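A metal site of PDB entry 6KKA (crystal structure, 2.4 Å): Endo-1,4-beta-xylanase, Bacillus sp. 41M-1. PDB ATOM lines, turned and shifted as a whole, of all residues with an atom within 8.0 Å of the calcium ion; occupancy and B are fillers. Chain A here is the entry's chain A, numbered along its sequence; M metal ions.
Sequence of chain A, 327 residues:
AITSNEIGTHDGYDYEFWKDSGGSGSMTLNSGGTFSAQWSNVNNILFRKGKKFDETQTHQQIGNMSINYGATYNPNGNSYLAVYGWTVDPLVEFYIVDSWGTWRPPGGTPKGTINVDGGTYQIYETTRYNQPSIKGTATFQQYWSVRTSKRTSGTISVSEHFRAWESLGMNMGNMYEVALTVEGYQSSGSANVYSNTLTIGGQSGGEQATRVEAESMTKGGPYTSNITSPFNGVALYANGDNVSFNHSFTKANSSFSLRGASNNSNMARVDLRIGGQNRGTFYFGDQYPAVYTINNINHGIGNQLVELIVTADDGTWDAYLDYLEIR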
ATOM      1  N   ARG A 211      26.686   1.333  16.130  1.00  0.00           N
ATOM      2  CA  ARG A 211      26.449   0.960  17.520  1.00  0.00           C
ATOM      3  C   ARG A 211      25.911  -0.460  17.602  1.00  0.00           C
ATOM      4  O   ARG A 211      24.882  -0.779  16.996  1.00  0.00           O
ATOM      5  CB  ARG A 211      25.445   1.909  18.186  1.00  0.00           C
ATOM      6  CG  ARG A 211      25.144   1.508  19.631  1.00  0.00           C
ATOM      7  CD  ARG A 211      24.176   2.437  20.326  1.00  0.00           C
ATOM      8  NE  ARG A 211      24.762   3.768  20.449  1.00  0.00           N
ATOM      9  CZ  ARG A 211      24.234   4.748  21.176  1.00  0.00           C
ATOM     10  NH1 ARG A 211      23.099   4.551  21.843  1.00  0.00           N
ATOM     11  NH2 ARG A 211      24.838   5.938  21.220  1.00  0.00           N
ATOM     12  N   VAL A 212      26.570  -1.306  18.385  1.00  0.00           N
ATOM     13  CA  VAL A 212      26.117  -2.682  18.630  1.00  0.00           C
ATOM     14  C   VAL A 212      25.764  -2.824  20.103  1.00  0.00           C
ATOM     15  O   VAL A 212      26.654  -2.730  20.957  1.00  0.00           O
ATOM     16  CB  VAL A 212      27.172  -3.723  18.219  1.00  0.00           C
ATOM     17  CG1 VAL A 212      26.624  -5.137  18.465  1.00  0.00           C
ATOM     18  CG2 VAL A 212      27.617  -3.522  16.751  1.00  0.00           C
ATOM     19  N   GLU A 213      24.487  -3.100  20.393  1.00  0.00           N
ATOM     20  CA  GLU A 213      24.035  -3.289  21.769  1.00  0.00           C
ATOM     21  C   GLU A 213      24.613  -4.571  22.356  1.00  0.00           C
ATOM     22  O   GLU A 213      24.561  -5.629  21.734  1.00  0.00           O
ATOM     23  CB  GLU A 213      22.511  -3.326  21.834  1.00  0.00           C
ATOM     24  CG  GLU A 213      21.837  -2.093  21.214  1.00  0.00           C
ATOM     25  CD  GLU A 213      21.999  -0.826  22.038  1.00  0.00           C
ATOM     26  OE1 GLU A 213      21.848   0.290  21.504  1.00  0.00           O
ATOM     27  OE2 GLU A 213      22.317  -0.954  23.230  1.00  0.00           O
ATOM     28  N   ALA A 214      25.158  -4.462  23.579  1.00  0.00           N
ATOM     29  CA  ALA A 214      25.816  -5.604  24.199  1.00  0.00           C
ATOM     30  C   ALA A 214      24.879  -6.799  24.349  1.00  0.00           C
ATOM     31  O   ALA A 214      25.334  -7.950  24.282  1.00  0.00           O
ATOM     32  CB  ALA A 214      26.371  -5.207  25.565  1.00  0.00           C
ATOM     33  N   GLU A 215      23.593  -6.555  24.597  1.00  0.00           N
ATOM     34  CA  GLU A 215      22.664  -7.657  24.808  1.00  0.00           C
ATOM     35  C   GLU A 215      22.329  -8.370  23.505  1.00  0.00           C
ATOM     36  O   GLU A 215      21.776  -9.471  23.550  1.00  0.00           O
ATOM     37  CB  GLU A 215      21.354  -7.179  25.476  1.00  0.00           C
ATOM     38  CG  GLU A 215      20.522  -6.240  24.606  1.00  0.00           C
ATOM     39  CD  GLU A 215      20.855  -4.766  24.820  1.00  0.00           C
ATOM     40  OE1 GLU A 215      20.020  -3.900  24.519  1.00  0.00           O
ATOM     41  OE2 GLU A 215      21.992  -4.477  25.274  1.00  0.00           O
ATOM     42  N   SER A 216      22.669  -7.791  22.368  1.00  0.00           N
ATOM     43  CA  SER A 216      22.467  -8.443  21.088  1.00  0.00           C
ATOM     44  C   SER A 216      23.722  -9.188  20.605  1.00  0.00           C
ATOM     45  O   SER A 216      23.678  -9.794  19.541  1.00  0.00           O
ATOM     46  CB  SER A 216      22.035  -7.406  20.049  1.00  0.00           C
ATOM     47  OG  SER A 216      23.176  -6.797  19.469  1.00  0.00           O
ATOM     48  N   MET A 217      24.811  -9.170  21.357  1.00  0.00           N
ATOM     49  CA  MET A 217      25.999  -9.905  20.961  1.00  0.00           C
ATOM     50  C   MET A 217      25.887 -11.352  21.446  1.00  0.00           C
ATOM     51  O   MET A 217      24.946 -11.722  22.143  1.00  0.00           O
ATOM     52  CB  MET A 217      27.264  -9.254  21.517  1.00  0.00           C
ATOM     53  CG  MET A 217      27.433  -7.762  21.267  1.00  0.00           C
ATOM     54  SD  MET A 217      28.805  -6.999  22.220  1.00  0.00           S
ATOM     55  CE  MET A 217      28.557  -5.301  21.699  1.00  0.00           C
ATOM     56  N   ILE A 227      21.012  -7.788  31.772  1.00  0.00           N
ATOM     57  CA  ILE A 227      20.614  -6.905  32.864  1.00  0.00           C
ATOM     58  C   ILE A 227      19.778  -5.776  32.282  1.00  0.00           C
ATOM     59  O   ILE A 227      19.844  -5.457  31.104  1.00  0.00           O
ATOM     60  CB  ILE A 227      21.819  -6.294  33.647  1.00  0.00           C
ATOM     61  CG1 ILE A 227      22.720  -5.469  32.717  1.00  0.00           C
ATOM     62  CG2 ILE A 227      22.594  -7.370  34.376  1.00  0.00           C
ATOM     63  CD1 ILE A 227      23.935  -4.893  33.417  1.00  0.00           C
ATOM     64  N   PHE A 231      21.337  -0.081  32.833  1.00  0.00           N
ATOM     65  CA  PHE A 231      20.911   0.077  31.451  1.00  0.00           C
ATOM     66  C   PHE A 231      20.544  -1.300  30.945  1.00  0.00           C
ATOM     67  O   PHE A 231      20.826  -2.311  31.590  1.00  0.00           O
ATOM     68  CB  PHE A 231      21.993   0.750  30.569  1.00  0.00           C
ATOM     69  CG  PHE A 231      23.400   0.297  30.897  1.00  0.00           C
ATOM     70  CD1 PHE A 231      23.757  -1.050  30.846  1.00  0.00           C
ATOM     71  CD2 PHE A 231      24.372   1.224  31.241  1.00  0.00           C
ATOM     72  CE1 PHE A 231      25.058  -1.481  31.149  1.00  0.00           C
ATOM     73  CE2 PHE A 231      25.690   0.812  31.555  1.00  0.00           C
ATOM     74  CZ  PHE A 231      26.028  -0.546  31.499  1.00  0.00           C
ATOM     75  N   ASN A 232      19.919  -1.339  29.768  1.00  0.00           N
ATOM     76  CA  ASN A 232      19.708  -2.616  29.103  1.00  0.00           C
ATOM     77  C   ASN A 232      21.037  -3.111  28.536  1.00  0.00           C
ATOM     78  O   ASN A 232      21.655  -2.442  27.704  1.00  0.00           O
ATOM     79  CB  ASN A 232      18.667  -2.448  27.997  1.00  0.00           C
ATOM     80  CG  ASN A 232      17.787  -3.666  27.854  1.00  0.00           C
ATOM     81  OD1 ASN A 232      17.369  -4.256  28.854  1.00  0.00           O
ATOM     82  ND2 ASN A 232      17.514  -4.068  26.611  1.00  0.00           N
ATOM     83  N   GLY A 233      21.495  -4.274  28.982  1.00  0.00           N
ATOM     84  CA  GLY A 233      22.808  -4.738  28.561  1.00  0.00           C
ATOM     85  C   GLY A 233      23.184  -6.092  29.129  1.00  0.00           C
ATOM     86  O   GLY A 233      22.335  -6.988  29.232  1.00  0.00           O
ATOM     87  N   VAL A 234      24.467  -6.293  29.453  1.00  0.00           N
ATOM     88  CA  VAL A 234      24.909  -7.565  30.009  1.00  0.00           C
ATOM     89  C   VAL A 234      25.881  -7.310  31.150  1.00  0.00           C
ATOM     90  O   VAL A 234      26.481  -6.243  31.277  1.00  0.00           O
ATOM     91  CB  VAL A 234      25.573  -8.507  28.960  1.00  0.00           C
ATOM     92  CG1 VAL A 234      24.754  -8.575  27.681  1.00  0.00           C
ATOM     93  CG2 VAL A 234      26.995  -8.059  28.689  1.00  0.00           C
ATOM     94  N   ARG A 259      30.241   1.766  26.230  1.00  0.00           N
ATOM     95  CA  ARG A 259      29.473   2.328  27.342  1.00  0.00           C
ATOM     96  C   ARG A 259      29.295   1.236  28.393  1.00  0.00           C
ATOM     97  O   ARG A 259      28.759   0.159  28.101  1.00  0.00           O
ATOM     98  CB  ARG A 259      28.117   2.860  26.912  1.00  0.00           C
ATOM     99  CG  ARG A 259      27.400   3.663  28.041  1.00  0.00           C
ATOM    100  CD  ARG A 259      26.291   4.561  27.507  1.00  0.00           C
ATOM    101  NE  ARG A 259      25.756   5.498  28.501  1.00  0.00           N
ATOM    102  CZ  ARG A 259      24.665   5.250  29.236  1.00  0.00           C
ATOM    103  NH1 ARG A 259      24.031   4.082  29.099  1.00  0.00           N
ATOM    104  NH2 ARG A 259      24.225   6.128  30.110  1.00  0.00           N
ATOM    105  N   LEU A 321      27.946  -3.884  30.693  1.00  0.00           N
ATOM    106  CA  LEU A 321      28.160  -3.351  29.360  1.00  0.00           C
ATOM    107  C   LEU A 321      26.828  -2.976  28.730  1.00  0.00           C
ATOM    108  O   LEU A 321      25.887  -3.774  28.735  1.00  0.00           O
ATOM    109  CB  LEU A 321      28.885  -4.362  28.464  1.00  0.00           C
ATOM    110  CG  LEU A 321      30.238  -4.769  29.024  1.00  0.00           C
ATOM    111  CD1 LEU A 321      30.895  -5.754  28.072  1.00  0.00           C
ATOM    112  CD2 LEU A 321      31.085  -3.536  29.159  1.00  0.00           C
ATOM    113  N   ASP A 322      26.763  -1.758  28.211  1.00  0.00           N
ATOM    114  CA  ASP A 322      25.562  -1.271  27.529  1.00  0.00           C
ATOM    115  C   ASP A 322      25.719  -1.548  26.027  1.00  0.00           C
ATOM    116  O   ASP A 322      25.012  -2.377  25.463  1.00  0.00           O
ATOM    117  CB  ASP A 322      25.361   0.205  27.838  1.00  0.00           C
ATOM    118  CG  ASP A 322      24.081   0.773  27.251  1.00  0.00           C
ATOM    119  OD1 ASP A 322      23.254   0.007  26.736  1.00  0.00           O
ATOM    120  OD2 ASP A 322      23.917   2.002  27.298  1.00  0.00           O
ATOM    121  N   TYR A 323      26.649  -0.852  25.378  1.00  0.00           N
ATOM    122  CA  TYR A 323      26.853  -1.014  23.948  1.00  0.00           C
ATOM    123  C   TYR A 323      28.291  -0.702  23.575  1.00  0.00           C
ATOM    124  O   TYR A 323      29.031  -0.059  24.334  1.00  0.00           O
ATOM    125  CB  TYR A 323      25.889  -0.123  23.131  1.00  0.00           C
ATOM    126  CG  TYR A 323      26.114   1.382  23.325  1.00  0.00           C
ATOM    127  CD1 TYR A 323      27.248   2.004  22.823  1.00  0.00           C
ATOM    128  CD2 TYR A 323      25.168   2.167  23.976  1.00  0.00           C
ATOM    129  CE1 TYR A 323      27.448   3.342  22.978  1.00  0.00           C
ATOM    130  CE2 TYR A 323      25.366   3.520  24.143  1.00  0.00           C
ATOM    131  CZ  TYR A 323      26.507   4.101  23.645  1.00  0.00           C
ATOM    132  OH  TYR A 323      26.727   5.435  23.792  1.00  0.00           O
ATOM    133  N   LEU A 324      28.676  -1.137  22.369  1.00  0.00           N
ATOM    134  CA  LEU A 324      29.961  -0.768  21.800  1.00  0.00           C
ATOM    135  C   LEU A 324      29.706  -0.042  20.483  1.00  0.00           C
ATOM    136  O   LEU A 324      28.964  -0.527  19.632  1.00  0.00           O
ATOM    137  CB  LEU A 324      30.855  -1.985  21.591  1.00  0.00           C
ATOM    138  CG  LEU A 324      32.227  -1.736  20.958  1.00  0.00           C
ATOM    139  CD1 LEU A 324      33.179  -1.066  21.931  1.00  0.00           C
ATOM    140  CD2 LEU A 324      32.823  -3.046  20.444  1.00  0.00           C
HETATM  141 CA    CA M   1      22.503  -1.975  25.431  1.00  0.00          CA
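The nearest printed residue that does not touch the calcium ion is Ala 214 (4.1 Å).
The calcium ion is bound by OE2 of Glu 213 (2.4 Å). The calcium ion is bound by O of Asn 232, 2.5 Å away. The calcium ion is bound by the side-chain carboxylate (OD1) of Asp 322 (2.5 Å). The calcium ion is bound by O of Asp 322, 2.5 Å away. The calcium ion is bound by OE2 of Glu 215.
The backbone carbonyl oxygen of Glu 213 sits at hydrogen-bond distance from the side-chain hydroxyl of Ser 216 (2.9 Å). The side-chain carboxylate (OD2) of Asp 322 is in salt-bridge range of the guanidinium group (NH1) of Arg 259 (2.8 Å). O of Asp 322 lies close to N of Ala 214 (2.8 Å).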
